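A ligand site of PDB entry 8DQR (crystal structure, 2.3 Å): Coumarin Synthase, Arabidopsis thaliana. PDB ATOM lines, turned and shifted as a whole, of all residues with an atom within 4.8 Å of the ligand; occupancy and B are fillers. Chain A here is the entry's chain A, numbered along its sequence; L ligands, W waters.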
ATOM      1  N   HIS A 161      15.977  15.064  -2.643  1.00  0.00           N
ATOM      2  CA  HIS A 161      14.874  15.695  -3.343  1.00  0.00           C
ATOM      3  C   HIS A 161      14.186  16.757  -2.473  1.00  0.00           C
ATOM      4  O   HIS A 161      13.439  17.576  -2.979  1.00  0.00           O
ATOM      5  CB  HIS A 161      13.907  14.615  -3.847  1.00  0.00           C
ATOM      6  CG  HIS A 161      13.060  15.054  -4.993  1.00  0.00           C
ATOM      7  ND1 HIS A 161      12.608  16.342  -5.137  1.00  0.00           N
ATOM      8  CD2 HIS A 161      12.541  14.352  -6.036  1.00  0.00           C
ATOM      9  CE1 HIS A 161      11.857  16.430  -6.222  1.00  0.00           C
ATOM     10  NE2 HIS A 161      11.797  15.231  -6.768  1.00  0.00           N
ATOM     11  N   ASP A 165      13.825  20.619  -6.753  1.00  0.00           N
ATOM     12  CA  ASP A 165      13.274  19.843  -7.879  1.00  0.00           C
ATOM     13  C   ASP A 165      14.282  19.839  -9.048  1.00  0.00           C
ATOM     14  O   ASP A 165      15.430  20.341  -8.960  1.00  0.00           O
ATOM     15  CB  ASP A 165      11.873  20.326  -8.264  1.00  0.00           C
ATOM     16  CG  ASP A 165      11.748  21.821  -8.481  1.00  0.00           C
ATOM     17  OD1 ASP A 165      12.784  22.469  -8.695  1.00  0.00           O
ATOM     18  OD2 ASP A 165      10.626  22.331  -8.417  1.00  0.00           O
ATOM     19  N   GLY A 166      13.847  19.229 -10.160  1.00  0.00           N
ATOM     20  CA  GLY A 166      14.615  19.210 -11.408  1.00  0.00           C
ATOM     21  C   GLY A 166      14.999  20.602 -11.878  1.00  0.00           C
ATOM     22  O   GLY A 166      16.150  20.806 -12.275  1.00  0.00           O
ATOM     23  N   LEU A 167      14.032  21.531 -11.822  1.00  0.00           N
ATOM     24  CA  LEU A 167      14.215  22.917 -12.226  1.00  0.00           C
ATOM     25  C   LEU A 167      15.185  23.625 -11.280  1.00  0.00           C
ATOM     26  O   LEU A 167      16.046  24.374 -11.742  1.00  0.00           O
ATOM     27  CB  LEU A 167      12.861  23.653 -12.238  1.00  0.00           C
ATOM     28  CG  LEU A 167      12.033  23.491 -13.510  1.00  0.00           C
ATOM     29  CD1 LEU A 167      10.564  23.614 -13.176  1.00  0.00           C
ATOM     30  CD2 LEU A 167      12.417  24.507 -14.589  1.00  0.00           C
ATOM     31  N   LYS A 246      -2.119  10.840 -32.766  1.00  0.00           N
ATOM     32  CA  LYS A 246      -2.835  12.099 -32.546  1.00  0.00           C
ATOM     33  C   LYS A 246      -3.993  12.268 -33.549  1.00  0.00           C
ATOM     34  O   LYS A 246      -5.068  12.764 -33.169  1.00  0.00           O
ATOM     35  CB  LYS A 246      -1.871  13.280 -32.624  1.00  0.00           C
ATOM     36  CG  LYS A 246      -1.002  13.461 -31.388  1.00  0.00           C
ATOM     37  CD  LYS A 246      -0.136  14.707 -31.432  1.00  0.00           C
ATOM     38  CE  LYS A 246       1.145  14.581 -30.661  1.00  0.00           C
ATOM     39  NZ  LYS A 246       1.702  15.905 -30.299  1.00  0.00           N
ATOM     40  N   PHE A 257      -4.707  16.307 -28.943  1.00  0.00           N
ATOM     41  CA  PHE A 257      -4.090  15.891 -27.751  1.00  0.00           C
ATOM     42  C   PHE A 257      -2.597  16.210 -27.819  1.00  0.00           C
ATOM     43  O   PHE A 257      -1.996  16.022 -28.850  1.00  0.00           O
ATOM     44  CB  PHE A 257      -4.276  14.392 -27.553  1.00  0.00           C
ATOM     45  CG  PHE A 257      -5.664  14.002 -27.142  1.00  0.00           C
ATOM     46  CD1 PHE A 257      -6.196  14.444 -25.946  1.00  0.00           C
ATOM     47  CD2 PHE A 257      -6.457  13.229 -27.966  1.00  0.00           C
ATOM     48  CE1 PHE A 257      -7.482  14.100 -25.580  1.00  0.00           C
ATOM     49  CE2 PHE A 257      -7.743  12.885 -27.600  1.00  0.00           C
ATOM     50  CZ  PHE A 257      -8.255  13.327 -26.404  1.00  0.00           C
ATOM     51  N   THR A 258      -2.038  16.653 -26.690  1.00  0.00           N
ATOM     52  CA  THR A 258      -0.604  16.742 -26.555  1.00  0.00           C
ATOM     53  C   THR A 258      -0.045  15.321 -26.601  1.00  0.00           C
ATOM     54  O   THR A 258      -0.783  14.341 -26.375  1.00  0.00           O
ATOM     55  CB  THR A 258      -0.186  17.485 -25.273  1.00  0.00           C
ATOM     56  OG1 THR A 258      -0.531  16.749 -24.089  1.00  0.00           O
ATOM     57  CG2 THR A 258      -0.796  18.866 -25.194  1.00  0.00           C
ATOM     58  N   THR A 259       1.244  15.217 -26.930  1.00  0.00           N
ATOM     59  CA  THR A 259       2.019  13.988 -26.825  1.00  0.00           C
ATOM     60  C   THR A 259       1.889  13.431 -25.391  1.00  0.00           C
ATOM     61  O   THR A 259       1.724  12.229 -25.176  1.00  0.00           O
ATOM     62  CB  THR A 259       3.454  14.280 -27.280  1.00  0.00           C
ATOM     63  OG1 THR A 259       3.404  14.297 -28.691  1.00  0.00           O
ATOM     64  CG2 THR A 259       4.484  13.257 -26.861  1.00  0.00           C
ATOM     65  N   PHE A 260       1.925  14.313 -24.399  1.00  0.00           N
ATOM     66  CA  PHE A 260       1.910  13.881 -23.023  1.00  0.00           C
ATOM     67  C   PHE A 260       0.572  13.210 -22.676  1.00  0.00           C
ATOM     68  O   PHE A 260       0.522  12.218 -22.011  1.00  0.00           O
ATOM     69  CB  PHE A 260       2.267  15.076 -22.133  1.00  0.00           C
ATOM     70  CG  PHE A 260       2.246  14.752 -20.674  1.00  0.00           C
ATOM     71  CD1 PHE A 260       3.319  14.111 -20.085  1.00  0.00           C
ATOM     72  CD2 PHE A 260       1.131  15.060 -19.905  1.00  0.00           C
ATOM     73  CE1 PHE A 260       3.289  13.795 -18.743  1.00  0.00           C
ATOM     74  CE2 PHE A 260       1.091  14.744 -18.563  1.00  0.00           C
ATOM     75  CZ  PHE A 260       2.174  14.098 -17.993  1.00  0.00           C
ATOM     76  N   GLU A 261      -0.515  13.778 -23.160  1.00  0.00           N
ATOM     77  CA  GLU A 261      -1.828  13.215 -22.939  1.00  0.00           C
ATOM     78  C   GLU A 261      -2.009  11.920 -23.758  1.00  0.00           C
ATOM     79  O   GLU A 261      -2.608  10.957 -23.277  1.00  0.00           O
ATOM     80  CB  GLU A 261      -2.909  14.222 -23.311  1.00  0.00           C
ATOM     81  CG  GLU A 261      -2.846  15.550 -22.574  1.00  0.00           C
ATOM     82  CD  GLU A 261      -3.590  16.692 -23.258  1.00  0.00           C
ATOM     83  OE1 GLU A 261      -3.826  16.599 -24.501  1.00  0.00           O
ATOM     84  OE2 GLU A 261      -3.950  17.672 -22.553  1.00  0.00           O
ATOM     85  N   TYR A 287       1.538  13.348 -12.178  1.00  0.00           N
ATOM     86  CA  TYR A 287       2.629  14.062 -12.766  1.00  0.00           C
ATOM     87  C   TYR A 287       2.859  15.331 -11.960  1.00  0.00           C
ATOM     88  O   TYR A 287       2.048  15.728 -11.135  1.00  0.00           O
ATOM     89  CB  TYR A 287       2.351  14.416 -14.233  1.00  0.00           C
ATOM     90  CG  TYR A 287       1.069  15.181 -14.461  1.00  0.00           C
ATOM     91  CD1 TYR A 287      -0.145  14.535 -14.403  1.00  0.00           C
ATOM     92  CD2 TYR A 287       1.071  16.543 -14.723  1.00  0.00           C
ATOM     93  CE1 TYR A 287      -1.340  15.220 -14.609  1.00  0.00           C
ATOM     94  CE2 TYR A 287      -0.103  17.243 -14.943  1.00  0.00           C
ATOM     95  CZ  TYR A 287      -1.309  16.575 -14.889  1.00  0.00           C
ATOM     96  OH  TYR A 287      -2.494  17.233 -15.076  1.00  0.00           O
ATOM     97  N   SER A 288       3.965  15.954 -12.323  1.00  0.00           N
ATOM     98  CA  SER A 288       4.571  17.038 -11.672  1.00  0.00           C
ATOM     99  C   SER A 288       4.502  18.278 -12.575  1.00  0.00           C
ATOM    100  O   SER A 288       5.140  18.289 -13.633  1.00  0.00           O
ATOM    101  CB  SER A 288       5.975  16.619 -11.421  1.00  0.00           C
ATOM    102  OG  SER A 288       6.569  17.451 -10.457  1.00  0.00           O
ATOM    103  N   ILE A 289       3.705  19.286 -12.189  1.00  0.00           N
ATOM    104  CA  ILE A 289       3.597  20.577 -12.888  1.00  0.00           C
ATOM    105  C   ILE A 289       4.410  21.624 -12.123  1.00  0.00           C
ATOM    106  O   ILE A 289       4.383  21.648 -10.901  1.00  0.00           O
ATOM    107  CB  ILE A 289       2.156  21.094 -13.022  1.00  0.00           C
ATOM    108  CG1 ILE A 289       1.363  20.996 -11.710  1.00  0.00           C
ATOM    109  CG2 ILE A 289       1.390  20.461 -14.147  1.00  0.00           C
ATOM    110  CD1 ILE A 289       0.496  22.238 -11.495  1.00  0.00           C
ATOM    111  N   ASN A 290       5.049  22.535 -12.881  1.00  0.00           N
ATOM    112  CA  ASN A 290       5.642  23.778 -12.402  1.00  0.00           C
ATOM    113  C   ASN A 290       4.511  24.707 -11.939  1.00  0.00           C
ATOM    114  O   ASN A 290       3.499  24.805 -12.630  1.00  0.00           O
ATOM    115  CB  ASN A 290       6.454  24.444 -13.516  1.00  0.00           C
ATOM    116  CG  ASN A 290       7.332  25.581 -13.038  1.00  0.00           C
ATOM    117  OD1 ASN A 290       7.805  25.578 -11.914  1.00  0.00           O
ATOM    118  ND2 ASN A 290       7.583  26.539 -13.902  1.00  0.00           N
ATOM    119  N   CSO A 308       7.063  22.470  -7.620  1.00  0.00           N
ATOM    120  CA  CSO A 308       6.274  21.551  -8.412  1.00  0.00           C
ATOM    121  CB  CSO A 308       7.291  20.507  -8.997  1.00  0.00           C
ATOM    122  SG  CSO A 308       7.638  20.928 -10.725  1.00  0.00           S
ATOM    123  C   CSO A 308       5.236  20.981  -7.429  1.00  0.00           C
ATOM    124  O   CSO A 308       5.448  20.971  -6.219  1.00  0.00           O
ATOM    125  OD  CSO A 308       9.295  20.982 -11.289  1.00  0.00           O
ATOM    126  N   LYS A 336      -5.347  18.700 -15.889  1.00  0.00           N
ATOM    127  CA  LYS A 336      -4.523  19.889 -15.957  1.00  0.00           C
ATOM    128  C   LYS A 336      -5.311  21.132 -15.514  1.00  0.00           C
ATOM    129  O   LYS A 336      -4.696  22.149 -15.272  1.00  0.00           O
ATOM    130  CB  LYS A 336      -3.928  20.054 -17.351  1.00  0.00           C
ATOM    131  CG  LYS A 336      -2.654  19.260 -17.583  1.00  0.00           C
ATOM    132  CD  LYS A 336      -2.476  18.680 -18.977  1.00  0.00           C
ATOM    133  CE  LYS A 336      -1.913  19.657 -19.983  1.00  0.00           C
ATOM    134  NZ  LYS A 336      -1.460  18.959 -21.208  1.00  0.00           N
ATOM    135  N   THR A 369       7.010  12.097 -15.711  1.00  0.00           N
ATOM    136  CA  THR A 369       7.813  13.297 -15.636  1.00  0.00           C
ATOM    137  C   THR A 369       8.334  13.601 -17.029  1.00  0.00           C
ATOM    138  O   THR A 369       8.969  12.778 -17.656  1.00  0.00           O
ATOM    139  CB  THR A 369       8.933  13.182 -14.597  1.00  0.00           C
ATOM    140  OG1 THR A 369       8.312  13.133 -13.309  1.00  0.00           O
ATOM    141  CG2 THR A 369       9.896  14.347 -14.586  1.00  0.00           C
ATOM    142  N   ASP A 370       8.011  14.799 -17.502  1.00  0.00           N
ATOM    143  CA  ASP A 370       8.436  15.260 -18.794  1.00  0.00           C
ATOM    144  C   ASP A 370       9.763  15.994 -18.607  1.00  0.00           C
ATOM    145  O   ASP A 370       9.817  17.054 -17.968  1.00  0.00           O
ATOM    146  CB  ASP A 370       7.352  16.135 -19.441  1.00  0.00           C
ATOM    147  CG  ASP A 370       7.624  16.482 -20.897  1.00  0.00           C
ATOM    148  OD1 ASP A 370       8.715  16.126 -21.402  1.00  0.00           O
ATOM    149  OD2 ASP A 370       6.750  17.107 -21.513  1.00  0.00           O
ATOM    150  N   ARG A 372      11.665  16.626 -21.372  1.00  0.00           N
ATOM    151  CA  ARG A 372      11.991  17.088 -22.747  1.00  0.00           C
ATOM    152  C   ARG A 372      12.495  18.546 -22.758  1.00  0.00           C
ATOM    153  O   ARG A 372      13.107  18.957 -23.734  1.00  0.00           O
ATOM    154  CB  ARG A 372      10.782  16.965 -23.686  1.00  0.00           C
ATOM    155  CG  ARG A 372      10.474  15.558 -24.191  1.00  0.00           C
ATOM    156  CD  ARG A 372       9.196  15.468 -25.024  1.00  0.00           C
ATOM    157  NE  ARG A 372       8.042  16.073 -24.352  1.00  0.00           N
ATOM    158  CZ  ARG A 372       6.820  16.200 -24.864  1.00  0.00           C
ATOM    159  NH1 ARG A 372       6.554  15.820 -26.096  1.00  0.00           N
ATOM    160  NH2 ARG A 372       5.842  16.688 -24.106  1.00  0.00           N
ATOM    161  N   TYR A 373      12.186  19.321 -21.712  1.00  0.00           N
ATOM    162  CA  TYR A 373      12.637  20.745 -21.524  1.00  0.00           C
ATOM    163  C   TYR A 373      13.520  20.783 -20.278  1.00  0.00           C
ATOM    164  O   TYR A 373      14.450  19.954 -20.176  1.00  0.00           O
ATOM    165  CB  TYR A 373      11.399  21.639 -21.624  1.00  0.00           C
ATOM    166  CG  TYR A 373      10.542  21.253 -22.810  1.00  0.00           C
ATOM    167  CD1 TYR A 373      11.106  21.126 -24.067  1.00  0.00           C
ATOM    168  CD2 TYR A 373       9.199  20.926 -22.678  1.00  0.00           C
ATOM    169  CE1 TYR A 373      10.368  20.716 -25.173  1.00  0.00           C
ATOM    170  CE2 TYR A 373       8.431  20.521 -23.776  1.00  0.00           C
ATOM    171  CZ  TYR A 373       9.026  20.414 -25.028  1.00  0.00           C
ATOM    172  OH  TYR A 373       8.329  20.051 -26.149  1.00  0.00           O
ATOM    173  N   LEU A 374      13.307  21.701 -19.337  1.00  0.00           N
ATOM    174  CA  LEU A 374      14.057  21.648 -17.991  1.00  0.00           C
ATOM    175  C   LEU A 374      15.471  22.272 -18.095  1.00  0.00           C
ATOM    176  O   LEU A 374      16.078  22.644 -17.029  1.00  0.00           O
ATOM    177  CB  LEU A 374      14.141  20.191 -17.473  1.00  0.00           C
ATOM    178  CG  LEU A 374      14.114  20.001 -15.949  1.00  0.00           C
ATOM    179  CD1 LEU A 374      12.732  19.532 -15.484  1.00  0.00           C
ATOM    180  CD2 LEU A 374      15.175  19.009 -15.456  1.00  0.00           C
HETATM  181  N1  LIG L   1       9.597  24.301 -26.424  1.00  0.00           N
HETATM  182  C1  LIG L   1       8.893  23.748 -27.447  1.00  0.00           C
HETATM  183  N2  LIG L   1       7.699  23.156 -27.239  1.00  0.00           N
HETATM  184  C2  LIG L   1       7.159  23.118 -25.975  1.00  0.00           C
HETATM  185  C3  LIG L   1       7.852  23.691 -24.812  1.00  0.00           C
HETATM  186  C4  LIG L   1       9.168  24.311 -25.123  1.00  0.00           C
HETATM  187  N3  LIG L   1       9.902  24.871 -24.143  1.00  0.00           N
HETATM  188  N4  LIG L   1       7.067  23.478 -23.716  1.00  0.00           N
HETATM  189  C5  LIG L   1       5.955  22.812 -24.142  1.00  0.00           C
HETATM  190  N5  LIG L   1       6.026  22.605 -25.488  1.00  0.00           N
HETATM  191  C6  LIG L   1       5.077  21.939 -26.394  1.00  0.00           C
HETATM  192  C7  LIG L   1       4.822  20.507 -25.976  1.00  0.00           C
HETATM  193  O1  LIG L   1       5.813  19.593 -26.515  1.00  0.00           O
HETATM  194  C8  LIG L   1       3.387  20.301 -26.442  1.00  0.00           C
HETATM  195  O2  LIG L   1       3.289  19.835 -27.805  1.00  0.00           O
HETATM  196  P1  LIG L   1       3.566  18.311 -28.133  1.00  0.00           P
HETATM  197  O3  LIG L   1       4.408  17.728 -27.018  1.00  0.00           O
HETATM  198  O4  LIG L   1       2.195  17.740 -28.305  1.00  0.00           O
HETATM  199  O5  LIG L   1       4.430  18.464 -29.316  1.00  0.00           O
HETATM  200  C9  LIG L   1       2.777  21.699 -26.378  1.00  0.00           C
HETATM  201  O6  LIG L   1       3.841  22.619 -26.369  1.00  0.00           O
HETATM  202  C10 LIG L   1       1.948  21.963 -25.150  1.00  0.00           C
HETATM  203  O7  LIG L   1       2.743  21.747 -23.965  1.00  0.00           O
HETATM  204  P2  LIG L   1       1.958  21.905 -22.560  1.00  0.00           P
HETATM  205  O8  LIG L   1       0.804  22.859 -22.802  1.00  0.00           O
HETATM  206  O9  LIG L   1       2.939  22.108 -21.414  1.00  0.00           O
HETATM  207  O10 LIG L   1       1.146  20.499 -22.449  1.00  0.00           O
HETATM  208  P3  LIG L   1       1.813  19.075 -22.203  1.00  0.00           P
HETATM  209  O11 LIG L   1       0.637  18.143 -22.052  1.00  0.00           O
HETATM  210  O12 LIG L   1       2.868  18.733 -23.201  1.00  0.00           O
HETATM  211  O13 LIG L   1       2.611  19.250 -20.820  1.00  0.00           O
HETATM  212  C11 LIG L   1       3.022  19.156 -18.409  1.00  0.00           C
HETATM  213  C12 LIG L   1       2.012  18.967 -19.547  1.00  0.00           C
HETATM  214  C13 LIG L   1       2.205  19.235 -17.137  1.00  0.00           C
HETATM  215  C14 LIG L   1       3.928  17.948 -18.320  1.00  0.00           C
HETATM  216  C15 LIG L   1       3.900  20.447 -18.549  1.00  0.00           C
HETATM  217  O14 LIG L   1       3.093  21.571 -18.873  1.00  0.00           O
HETATM  218  C16 LIG L   1       4.647  20.856 -17.296  1.00  0.00           C
HETATM  219  O15 LIG L   1       4.096  21.556 -16.435  1.00  0.00           O
HETATM  220  N6  LIG L   1       5.912  20.445 -17.181  1.00  0.00           N
HETATM  221  C17 LIG L   1       6.797  20.757 -16.067  1.00  0.00           C
HETATM  222  C18 LIG L   1       7.488  19.481 -15.636  1.00  0.00           C
HETATM  223  C19 LIG L   1       8.792  19.687 -14.899  1.00  0.00           C
HETATM  224  O16 LIG L   1       9.575  20.524 -15.323  1.00  0.00           O
HETATM  225  N7  LIG L   1       9.015  18.857 -13.856  1.00  0.00           N
HETATM  226  C20 LIG L   1      10.305  18.701 -13.149  1.00  0.00           C
HETATM  227  C21 LIG L   1      10.140  18.283 -11.672  1.00  0.00           C
HETATM  228  S1  LIG L   1      11.342  17.076 -10.971  1.00  0.00           S
HETATM  229  O   HOH W   1       5.924  16.653 -15.638  1.00  0.00           O
HETATM  230  O   HOH W   2       8.976  26.461 -28.103  1.00  0.00           O
HETATM  231  O   HOH W   3       3.433  16.877 -24.954  1.00  0.00           O
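The side-chain hydroxyl (OH) of Tyr 287 lies close to the backbone NH (N) of Lys 336, 3.3 Å away. OE2 of Glu 261 is in salt-bridge range of NZ of Lys 336, at 3.1 Å. The side-chain hydroxyl of Thr 258 lies close to the backbone NH of Phe 260. N of Thr 258 lies within hydrogen-bond range of OE1 of Glu 261 (2.8 Å). The side-chain amino group (NZ) of Lys 246 sits at hydrogen-bond distance from the side-chain hydroxyl (OG1) of Thr 259. OD of CSO 308 sits at hydrogen-bond distance from the side-chain carboxylate of Asp 165 (3.4 Å). The guanidinium group (NH2) of Arg 372 lies within salt-bridge range of the side-chain carboxylate (OD2) of Asp 370 (2.8 Å). The backbone NH (N) of Leu 167 sits close to the side-chain carboxylate (OD1) of Asp 165, at 3.5 Å.
O11 of the ligand lies within salt-bridge range of NZ of Lys 336 (2.4 Å). OH of Tyr 373 lies within hydrogen-bond range of O1 of the ligand, 2.6 Å away. OG1 of Thr 258 is in hydrogen-bond range of O11 of the ligand, 2.7 Å away. NZ of Lys 246 lies within salt-bridge range of O4 of the ligand (2.8 Å). A nitrogen (N7) of the ligand lies close to OD of CSO 308 (3.3 Å). NH1 of Arg 372 is in salt-bridge range of O3 of the ligand. An oxygen (O4) of the ligand sits at hydrogen-bond distance from the backbone NH (N) of Thr 259. S1 of the ligand sits close to N of Gly 166, at 3.4 Å.
CD1 of Leu 167 touches O16 of the ligand, 3.9 Å away. Phe 260 touches the ligand. Tyr 287 touches the ligand (CE2 to C13, 3.8 Å). Ser 288 touches the ligand. Ile 289 touches the ligand. Asn 290 touches the ligand (N to O15, 3.8 Å). CD1 of Leu 374 touches O16 of the ligand (3.3 Å). Hydrophobic or aromatic side chains that line the ligand: Leu 167, Phe 260, Tyr 287, Ile 289, Tyr 373 and Leu 374. The nearest printed residue that does not touch the ligand is Asp 370 (4.03 Å).
Water W1 bridges the backbone carbonyl oxygen (O) of Ser 288 and the backbone NH (N) of Asp 370.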
